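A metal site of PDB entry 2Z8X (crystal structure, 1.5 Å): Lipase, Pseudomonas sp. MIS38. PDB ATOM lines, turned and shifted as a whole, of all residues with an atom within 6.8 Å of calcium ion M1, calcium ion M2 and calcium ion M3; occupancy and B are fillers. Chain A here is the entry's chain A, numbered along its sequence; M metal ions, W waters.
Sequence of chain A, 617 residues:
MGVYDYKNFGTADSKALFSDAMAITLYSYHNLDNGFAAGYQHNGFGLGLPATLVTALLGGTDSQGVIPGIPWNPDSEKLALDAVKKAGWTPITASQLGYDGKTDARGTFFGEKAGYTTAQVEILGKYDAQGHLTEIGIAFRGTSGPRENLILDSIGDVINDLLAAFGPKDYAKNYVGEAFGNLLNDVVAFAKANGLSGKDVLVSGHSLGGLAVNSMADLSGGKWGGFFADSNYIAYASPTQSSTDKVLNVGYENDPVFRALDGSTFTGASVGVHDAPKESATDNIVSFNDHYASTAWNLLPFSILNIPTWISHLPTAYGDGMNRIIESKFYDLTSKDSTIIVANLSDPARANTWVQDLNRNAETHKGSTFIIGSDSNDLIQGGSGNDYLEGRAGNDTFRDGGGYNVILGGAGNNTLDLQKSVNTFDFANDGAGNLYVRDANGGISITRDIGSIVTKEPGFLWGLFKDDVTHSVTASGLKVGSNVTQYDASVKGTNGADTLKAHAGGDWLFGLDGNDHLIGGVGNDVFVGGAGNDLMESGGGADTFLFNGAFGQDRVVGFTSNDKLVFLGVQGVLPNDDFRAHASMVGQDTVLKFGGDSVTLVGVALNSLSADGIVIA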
ATOM      1  N   GLY A 493     -10.202   0.226 -14.748  1.00  0.00           N
ATOM      2  CA  GLY A 493     -11.014  -0.846 -14.215  1.00  0.00           C
ATOM      3  C   GLY A 493     -11.995  -1.385 -15.228  1.00  0.00           C
ATOM      4  O   GLY A 493     -11.723  -1.403 -16.444  1.00  0.00           O
ATOM      5  N   THR A 494     -13.127  -1.860 -14.726  1.00  0.00           N
ATOM      6  CA  THR A 494     -14.210  -2.391 -15.539  1.00  0.00           C
ATOM      7  C   THR A 494     -15.500  -1.750 -15.048  1.00  0.00           C
ATOM      8  O   THR A 494     -15.494  -0.957 -14.081  1.00  0.00           O
ATOM      9  CB  THR A 494     -14.337  -3.932 -15.376  1.00  0.00           C
ATOM     10  OG1 THR A 494     -14.807  -4.254 -14.058  1.00  0.00           O
ATOM     11  CG2 THR A 494     -13.000  -4.618 -15.621  1.00  0.00           C
ATOM     12  N   ASN A 495     -16.625  -2.094 -15.648  1.00  0.00           N
ATOM     13  CA  ASN A 495     -17.885  -1.570 -15.137  1.00  0.00           C
ATOM     14  C   ASN A 495     -18.470  -2.358 -13.966  1.00  0.00           C
ATOM     15  O   ASN A 495     -19.550  -2.073 -13.512  1.00  0.00           O
ATOM     16  CB  ASN A 495     -18.902  -1.405 -16.264  1.00  0.00           C
ATOM     17  CG  ASN A 495     -18.626  -0.202 -17.147  1.00  0.00           C
ATOM     18  OD1 ASN A 495     -18.199   0.842 -16.694  1.00  0.00           O
ATOM     19  ND2 ASN A 495     -18.895  -0.358 -18.424  1.00  0.00           N
ATOM     20  N   GLY A 496     -17.704  -3.321 -13.489  1.00  0.00           N
ATOM     21  CA  GLY A 496     -18.006  -3.982 -12.210  1.00  0.00           C
ATOM     22  C   GLY A 496     -17.142  -3.420 -11.090  1.00  0.00           C
ATOM     23  O   GLY A 496     -16.423  -2.435 -11.290  1.00  0.00           O
ATOM     24  N   ALA A 497     -17.222  -4.022  -9.902  1.00  0.00           N
ATOM     25  CA  ALA A 497     -16.410  -3.578  -8.763  1.00  0.00           C
ATOM     26  C   ALA A 497     -14.953  -4.027  -8.921  1.00  0.00           C
ATOM     27  O   ALA A 497     -14.674  -5.222  -9.085  1.00  0.00           O
ATOM     28  CB  ALA A 497     -17.002  -4.104  -7.465  1.00  0.00           C
ATOM     29  N   ASP A 498     -14.044  -3.057  -8.877  1.00  0.00           N
ATOM     30  CA  ASP A 498     -12.606  -3.318  -9.042  1.00  0.00           C
ATOM     31  C   ASP A 498     -11.809  -2.800  -7.869  1.00  0.00           C
ATOM     32  O   ASP A 498     -12.192  -1.819  -7.238  1.00  0.00           O
ATOM     33  CB  ASP A 498     -12.045  -2.608 -10.275  1.00  0.00           C
ATOM     34  CG  ASP A 498     -12.921  -2.749 -11.496  1.00  0.00           C
ATOM     35  OD1 ASP A 498     -13.072  -3.889 -11.977  1.00  0.00           O
ATOM     36  OD2 ASP A 498     -13.432  -1.699 -11.975  1.00  0.00           O
ATOM     37  N   LEU A 500      -8.126  -1.187  -7.798  1.00  0.00           N
ATOM     38  CA  LEU A 500      -7.057  -0.707  -8.682  1.00  0.00           C
ATOM     39  C   LEU A 500      -5.960  -0.128  -7.811  1.00  0.00           C
ATOM     40  O   LEU A 500      -6.232   0.623  -6.880  1.00  0.00           O
ATOM     41  CB  LEU A 500      -7.574   0.381  -9.635  1.00  0.00           C
ATOM     42  CG  LEU A 500      -8.759   0.043 -10.533  1.00  0.00           C
ATOM     43  CD1 LEU A 500      -9.014   1.226 -11.462  1.00  0.00           C
ATOM     44  CD2 LEU A 500      -8.511  -1.239 -11.318  1.00  0.00           C
ATOM     45  N   PHE A 510      -8.873   4.894 -13.118  1.00  0.00           N
ATOM     46  CA  PHE A 510     -10.215   5.013 -13.689  1.00  0.00           C
ATOM     47  C   PHE A 510     -11.093   3.845 -13.262  1.00  0.00           C
ATOM     48  O   PHE A 510     -11.035   2.760 -13.844  1.00  0.00           O
ATOM     49  CB  PHE A 510     -10.135   5.047 -15.222  1.00  0.00           C
ATOM     50  CG  PHE A 510      -9.384   6.226 -15.771  1.00  0.00           C
ATOM     51  CD1 PHE A 510      -9.896   7.516 -15.651  1.00  0.00           C
ATOM     52  CD2 PHE A 510      -8.196   6.035 -16.464  1.00  0.00           C
ATOM     53  CE1 PHE A 510      -9.224   8.599 -16.197  1.00  0.00           C
ATOM     54  CE2 PHE A 510      -7.522   7.104 -17.005  1.00  0.00           C
ATOM     55  CZ  PHE A 510      -8.031   8.397 -16.873  1.00  0.00           C
ATOM     56  N   GLY A 511     -11.938   4.073 -12.258  1.00  0.00           N
ATOM     57  CA  GLY A 511     -12.770   3.013 -11.724  1.00  0.00           C
ATOM     58  C   GLY A 511     -13.880   2.576 -12.665  1.00  0.00           C
ATOM     59  O   GLY A 511     -14.290   1.428 -12.648  1.00  0.00           O
ATOM     60  N   LEU A 512     -14.372   3.523 -13.467  1.00  0.00           N
ATOM     61  CA  LEU A 512     -15.565   3.299 -14.300  1.00  0.00           C
ATOM     62  C   LEU A 512     -16.776   2.910 -13.430  1.00  0.00           C
ATOM     63  O   LEU A 512     -16.814   3.231 -12.231  1.00  0.00           O
ATOM     64  CB  LEU A 512     -15.283   2.255 -15.387  1.00  0.00           C
ATOM     65  CG  LEU A 512     -14.003   2.447 -16.222  1.00  0.00           C
ATOM     66  CD1 LEU A 512     -13.826   1.284 -17.215  1.00  0.00           C
ATOM     67  CD2 LEU A 512     -13.965   3.821 -16.927  1.00  0.00           C
ATOM     68  N   ASP A 513     -17.776   2.228 -13.997  1.00  0.00           N
ATOM     69  CA  ASP A 513     -18.972   1.905 -13.213  1.00  0.00           C
ATOM     70  C   ASP A 513     -18.671   0.908 -12.087  1.00  0.00           C
ATOM     71  O   ASP A 513     -17.607   0.285 -12.074  1.00  0.00           O
ATOM     72  CB  ASP A 513     -20.095   1.349 -14.099  1.00  0.00           C
ATOM     73  CG  ASP A 513     -20.568   2.326 -15.175  1.00  0.00           C
ATOM     74  OD1 ASP A 513     -20.163   3.515 -15.202  1.00  0.00           O
ATOM     75  OD2 ASP A 513     -21.373   1.875 -16.023  1.00  0.00           O
ATOM     76  N   GLY A 514     -19.593   0.792 -11.148  1.00  0.00           N
ATOM     77  CA  GLY A 514     -19.443  -0.137 -10.033  1.00  0.00           C
ATOM     78  C   GLY A 514     -18.768   0.506  -8.836  1.00  0.00           C
ATOM     79  O   GLY A 514     -18.174   1.583  -8.948  1.00  0.00           O
ATOM     80  N   ASN A 515     -18.848  -0.161  -7.696  1.00  0.00           N
ATOM     81  CA  ASN A 515     -18.280   0.366  -6.451  1.00  0.00           C
ATOM     82  C   ASN A 515     -16.832  -0.059  -6.332  1.00  0.00           C
ATOM     83  O   ASN A 515     -16.529  -1.212  -5.982  1.00  0.00           O
ATOM     84  CB  ASN A 515     -19.074  -0.134  -5.245  1.00  0.00           C
ATOM     85  CG  ASN A 515     -20.549   0.260  -5.278  1.00  0.00           C
ATOM     86  OD1 ASN A 515     -20.959   1.187  -5.974  1.00  0.00           O
ATOM     87  ND2 ASN A 515     -21.352  -0.459  -4.513  1.00  0.00           N
ATOM     88  N   ASP A 516     -15.933   0.884  -6.597  1.00  0.00           N
ATOM     89  CA  ASP A 516     -14.529   0.559  -6.741  1.00  0.00           C
ATOM     90  C   ASP A 516     -13.693   0.923  -5.523  1.00  0.00           C
ATOM     91  O   ASP A 516     -14.108   1.720  -4.691  1.00  0.00           O
ATOM     92  CB  ASP A 516     -13.972   1.225  -7.997  1.00  0.00           C
ATOM     93  CG  ASP A 516     -14.749   0.818  -9.232  1.00  0.00           C
ATOM     94  OD1 ASP A 516     -14.853  -0.397  -9.473  1.00  0.00           O
ATOM     95  OD2 ASP A 516     -15.263   1.702  -9.933  1.00  0.00           O
ATOM     96  N   LEU A 518      -9.992   2.202  -4.936  1.00  0.00           N
ATOM     97  CA  LEU A 518      -8.853   2.788  -5.626  1.00  0.00           C
ATOM     98  C   LEU A 518      -7.739   3.094  -4.653  1.00  0.00           C
ATOM     99  O   LEU A 518      -7.890   3.972  -3.793  1.00  0.00           O
ATOM    100  CB  LEU A 518      -9.287   4.070  -6.363  1.00  0.00           C
ATOM    101  CG  LEU A 518      -9.827   3.946  -7.792  1.00  0.00           C
ATOM    102  CD1 LEU A 518     -10.734   2.758  -8.008  1.00  0.00           C
ATOM    103  CD2 LEU A 518     -10.462   5.239  -8.275  1.00  0.00           C
ATOM    104  N   VAL A 528     -10.370   8.912 -10.529  1.00  0.00           N
ATOM    105  CA  VAL A 528     -11.661   9.099 -11.172  1.00  0.00           C
ATOM    106  C   VAL A 528     -12.509   7.872 -10.834  1.00  0.00           C
ATOM    107  O   VAL A 528     -12.506   6.864 -11.570  1.00  0.00           O
ATOM    108  CB  VAL A 528     -11.533   9.304 -12.694  1.00  0.00           C
ATOM    109  CG1 VAL A 528     -12.882   9.736 -13.252  1.00  0.00           C
ATOM    110  CG2 VAL A 528     -10.494  10.368 -13.001  1.00  0.00           C
ATOM    111  N   GLY A 529     -13.225   7.946  -9.718  1.00  0.00           N
ATOM    112  CA  GLY A 529     -14.032   6.819  -9.253  1.00  0.00           C
ATOM    113  C   GLY A 529     -15.102   6.439 -10.268  1.00  0.00           C
ATOM    114  O   GLY A 529     -15.440   5.255 -10.412  1.00  0.00           O
ATOM    115  N   GLY A 530     -15.634   7.448 -10.942  1.00  0.00           N
ATOM    116  CA  GLY A 530     -16.736   7.244 -11.896  1.00  0.00           C
ATOM    117  C   GLY A 530     -18.050   6.958 -11.199  1.00  0.00           C
ATOM    118  O   GLY A 530     -18.223   7.240 -10.005  1.00  0.00           O
ATOM    119  N   ALA A 531     -19.000   6.401 -11.946  1.00  0.00           N
ATOM    120  CA  ALA A 531     -20.264   5.981 -11.351  1.00  0.00           C
ATOM    121  C   ALA A 531     -20.011   4.948 -10.255  1.00  0.00           C
ATOM    122  O   ALA A 531     -18.948   4.297 -10.210  1.00  0.00           O
ATOM    123  CB  ALA A 531     -21.184   5.415 -12.409  1.00  0.00           C
ATOM    124  N   GLY A 532     -20.985   4.823  -9.353  1.00  0.00           N
ATOM    125  CA  GLY A 532     -20.878   3.903  -8.245  1.00  0.00           C
ATOM    126  C   GLY A 532     -20.263   4.580  -7.035  1.00  0.00           C
ATOM    127  O   GLY A 532     -19.823   5.735  -7.092  1.00  0.00           O
ATOM    128  N   ASN A 533     -20.236   3.841  -5.931  1.00  0.00           N
ATOM    129  CA  ASN A 533     -19.783   4.372  -4.650  1.00  0.00           C
ATOM    130  C   ASN A 533     -18.362   3.894  -4.447  1.00  0.00           C
ATOM    131  O   ASN A 533     -18.134   2.719  -4.146  1.00  0.00           O
ATOM    132  CB  ASN A 533     -20.690   3.877  -3.515  1.00  0.00           C
ATOM    133  CG  ASN A 533     -22.144   4.291  -3.697  1.00  0.00           C
ATOM    134  OD1 ASN A 533     -22.457   5.219  -4.456  1.00  0.00           O
ATOM    135  ND2 ASN A 533     -23.038   3.603  -2.994  1.00  0.00           N
ATOM    136  N   ASP A 534     -17.417   4.808  -4.622  1.00  0.00           N
ATOM    137  CA  ASP A 534     -16.021   4.429  -4.687  1.00  0.00           C
ATOM    138  C   ASP A 534     -15.260   4.831  -3.439  1.00  0.00           C
ATOM    139  O   ASP A 534     -15.466   5.923  -2.904  1.00  0.00           O
ATOM    140  CB  ASP A 534     -15.376   5.035  -5.933  1.00  0.00           C
ATOM    141  CG  ASP A 534     -16.123   4.688  -7.202  1.00  0.00           C
ATOM    142  OD1 ASP A 534     -16.101   3.510  -7.624  1.00  0.00           O
ATOM    143  OD2 ASP A 534     -16.748   5.587  -7.779  1.00  0.00           O
ATOM    144  N   MET A 536     -11.595   5.678  -2.161  1.00  0.00           N
ATOM    145  CA  MET A 536     -10.380   6.156  -2.815  1.00  0.00           C
ATOM    146  C   MET A 536      -9.375   6.627  -1.765  1.00  0.00           C
ATOM    147  O   MET A 536      -9.672   7.527  -0.980  1.00  0.00           O
ATOM    148  CB  MET A 536     -10.748   7.284  -3.789  1.00  0.00           C
ATOM    149  CG  MET A 536     -11.762   6.792  -4.837  1.00  0.00           C
ATOM    150  SD  MET A 536     -12.234   8.033  -6.024  1.00  0.00           S
ATOM    151  CE  MET A 536     -13.484   8.918  -5.124  1.00  0.00           C
ATOM    152  N   PHE A 547     -14.614  14.469  -9.906  1.00  0.00           N
ATOM    153  CA  PHE A 547     -16.014  14.047  -9.771  1.00  0.00           C
ATOM    154  C   PHE A 547     -16.835  14.690 -10.874  1.00  0.00           C
ATOM    155  O   PHE A 547     -16.836  15.905 -11.017  1.00  0.00           O
ATOM    156  CB  PHE A 547     -16.564  14.428  -8.387  1.00  0.00           C
ATOM    157  CG  PHE A 547     -15.729  13.937  -7.250  1.00  0.00           C
ATOM    158  CD1 PHE A 547     -15.906  12.648  -6.741  1.00  0.00           C
ATOM    159  CD2 PHE A 547     -14.729  14.746  -6.707  1.00  0.00           C
ATOM    160  CE1 PHE A 547     -15.110  12.183  -5.708  1.00  0.00           C
ATOM    161  CE2 PHE A 547     -13.934  14.280  -5.674  1.00  0.00           C
ATOM    162  CZ  PHE A 547     -14.123  12.996  -5.170  1.00  0.00           C
ATOM    163  N   ALA A 550     -23.329  11.899 -12.328  1.00  0.00           N
ATOM    164  CA  ALA A 550     -23.969  11.266 -11.182  1.00  0.00           C
ATOM    165  C   ALA A 550     -22.930  10.344 -10.537  1.00  0.00           C
ATOM    166  O   ALA A 550     -22.927   9.122 -10.766  1.00  0.00           O
ATOM    167  CB  ALA A 550     -25.211  10.496 -11.621  1.00  0.00           C
ATOM    168  N   PHE A 551     -22.055  10.947  -9.754  1.00  0.00           N
ATOM    169  CA  PHE A 551     -20.826  10.280  -9.328  1.00  0.00           C
ATOM    170  C   PHE A 551     -20.968   9.370  -8.106  1.00  0.00           C
ATOM    171  O   PHE A 551     -20.013   8.694  -7.736  1.00  0.00           O
ATOM    172  CB  PHE A 551     -19.664  11.278  -9.152  1.00  0.00           C
ATOM    173  CG  PHE A 551     -19.887  12.303  -8.082  1.00  0.00           C
ATOM    174  CD1 PHE A 551     -20.362  13.571  -8.400  1.00  0.00           C
ATOM    175  CD2 PHE A 551     -19.599  12.009  -6.756  1.00  0.00           C
ATOM    176  CE1 PHE A 551     -20.568  14.522  -7.388  1.00  0.00           C
ATOM    177  CE2 PHE A 551     -19.816  12.942  -5.750  1.00  0.00           C
ATOM    178  CZ  PHE A 551     -20.292  14.202  -6.073  1.00  0.00           C
ATOM    179  N   GLY A 552     -22.160   9.346  -7.498  1.00  0.00           N
ATOM    180  CA  GLY A 552     -22.419   8.403  -6.402  1.00  0.00           C
ATOM    181  C   GLY A 552     -22.033   8.916  -5.029  1.00  0.00           C
ATOM    182  O   GLY A 552     -21.948  10.127  -4.820  1.00  0.00           O
ATOM    183  N   GLN A 553     -21.858   7.977  -4.093  1.00  0.00           N
ATOM    184  CA  GLN A 553     -21.496   8.319  -2.714  1.00  0.00           C
ATOM    185  C   GLN A 553     -20.096   7.780  -2.480  1.00  0.00           C
ATOM    186  O   GLN A 553     -19.907   6.583  -2.216  1.00  0.00           O
ATOM    187  CB  GLN A 553     -22.459   7.714  -1.684  1.00  0.00           C
ATOM    188  CG  GLN A 553     -23.901   7.559  -2.167  1.00  0.00           C
ATOM    189  CD  GLN A 553     -24.551   8.879  -2.547  1.00  0.00           C
ATOM    190  OE1 GLN A 553     -25.279   8.951  -3.538  1.00  0.00           O
ATOM    191  NE2 GLN A 553     -24.310   9.909  -1.752  1.00  0.00           N
ATOM    192  N   ASP A 554     -19.117   8.669  -2.573  1.00  0.00           N
ATOM    193  CA  ASP A 554     -17.710   8.286  -2.525  1.00  0.00           C
ATOM    194  C   ASP A 554     -17.121   8.585  -1.154  1.00  0.00           C
ATOM    195  O   ASP A 554     -17.593   9.443  -0.448  1.00  0.00           O
ATOM    196  CB  ASP A 554     -16.935   9.079  -3.572  1.00  0.00           C
ATOM    197  CG  ASP A 554     -17.362   8.778  -4.992  1.00  0.00           C
ATOM    198  OD1 ASP A 554     -17.761   7.620  -5.280  1.00  0.00           O
ATOM    199  OD2 ASP A 554     -17.247   9.706  -5.817  1.00  0.00           O
ATOM    200  N   SER A 598     -22.452  12.475  -3.228  1.00  0.00           N
ATOM    201  CA  SER A 598     -21.678  12.999  -2.104  1.00  0.00           C
ATOM    202  C   SER A 598     -20.252  12.488  -2.075  1.00  0.00           C
ATOM    203  O   SER A 598     -19.957  11.397  -2.588  1.00  0.00           O
ATOM    204  CB  SER A 598     -22.339  12.654  -0.767  1.00  0.00           C
ATOM    205  OG  SER A 598     -22.296  11.248  -0.530  1.00  0.00           O
HETATM  206 CA    CA M   1     -18.198   7.408  -7.678  1.00  0.00          CA
HETATM  207 CA    CA M   2     -16.845   3.418  -9.841  1.00  0.00          CA
HETATM  208 CA    CA M   3     -15.406  -0.422 -11.814  1.00  0.00          CA
HETATM  209  O   HOH W   1     -16.481   8.974  -8.208  1.00  0.00           O
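The backbone NH (N) of Gly 511 sits at hydrogen-bond distance from the backbone carbonyl oxygen (O) of Val 528 (2.9 Å).
The backbone NH (N) of Gly 496 is in hydrogen-bond range of the side-chain hydroxyl (OG1) of Thr 494.
The backbone NH (N) of Asp 513 sits at hydrogen-bond distance from the side-chain amide oxygen (OD1) of Asn 495, 3.1 Å away.
The backbone carbonyl oxygen of Ser 598 sits at hydrogen-bond distance from the backbone NH of Asp 554 (2.9 Å).
Six residues have an atom within 4 Å of calcium ion M1: Gly 530, Ala 531, Gly 532, Asp 534, Phe 551 and Asp 554.
Along chain A the residues within 4 Å of calcium ion M1 span positions 530 to 554.
Eight residues have an atom within 4 Å of calcium ion M2: Leu 512, Asp 513, Gly 514, Asp 516, Gly 529, Gly 530, Ala 531 and Asp 534.
Of the 30 residues printed, 7 come within 4 Å of calcium ion M3.
The nearest printed residue that does not touch calcium ion M3 is Asn 495 (4.2 Å).
Calcium ion M1 is bound by O of Phe 551 (2.2 Å), OD2 of Asp 534 (2.3 Å), O of Gly 530 (2.3 Å), water W1 (2.4 Å), O of Gly 532 (2.4 Å) and OD1 of Asp 554 (2.4 Å).
Calcium ion M1 has six donor atoms within binding distance.
Slightly farther from calcium ion M1 lies OD2 of Asp 554 (3.1 Å).
Calcium ion M2 is bound by the backbone carbonyl oxygen of Ala 531 (2.3 Å), the side-chain carboxylate of Asp 516 (2.3 Å), the side-chain carboxylate of Asp 534 (2.3 Å), the backbone carbonyl oxygen of Gly 529 (2.4 Å), the backbone carbonyl oxygen of Leu 512 (2.4 Å) and the backbone carbonyl oxygen of Gly 514 (2.4 Å).
Slightly farther from calcium ion M2 lies OD2 of Asp 534 (3.0 Å).
Calcium ion M3 is bound by O of Gly 511 (2.3 Å).
O of Gly 496 is bound to calcium ion M3, 2.3 Å away.
The backbone carbonyl oxygen (O) of Asp 513 is bound to calcium ion M3, 2.3 Å away.
O of Thr 494 binds calcium ion M3 (2.3 Å).
The side-chain carboxylate (OD2) of Asp 498 is bound to calcium ion M3 (2.4 Å).
The side-chain carboxylate (OD1) of Asp 516 is bound to calcium ion M3, at 2.4 Å.
OD2 of Asp 516 is bound to calcium ion M3, 2.8 Å away.
Water W1 lies within hydrogen-bond range of OD2 of Asp 554 and N of Gly 530.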
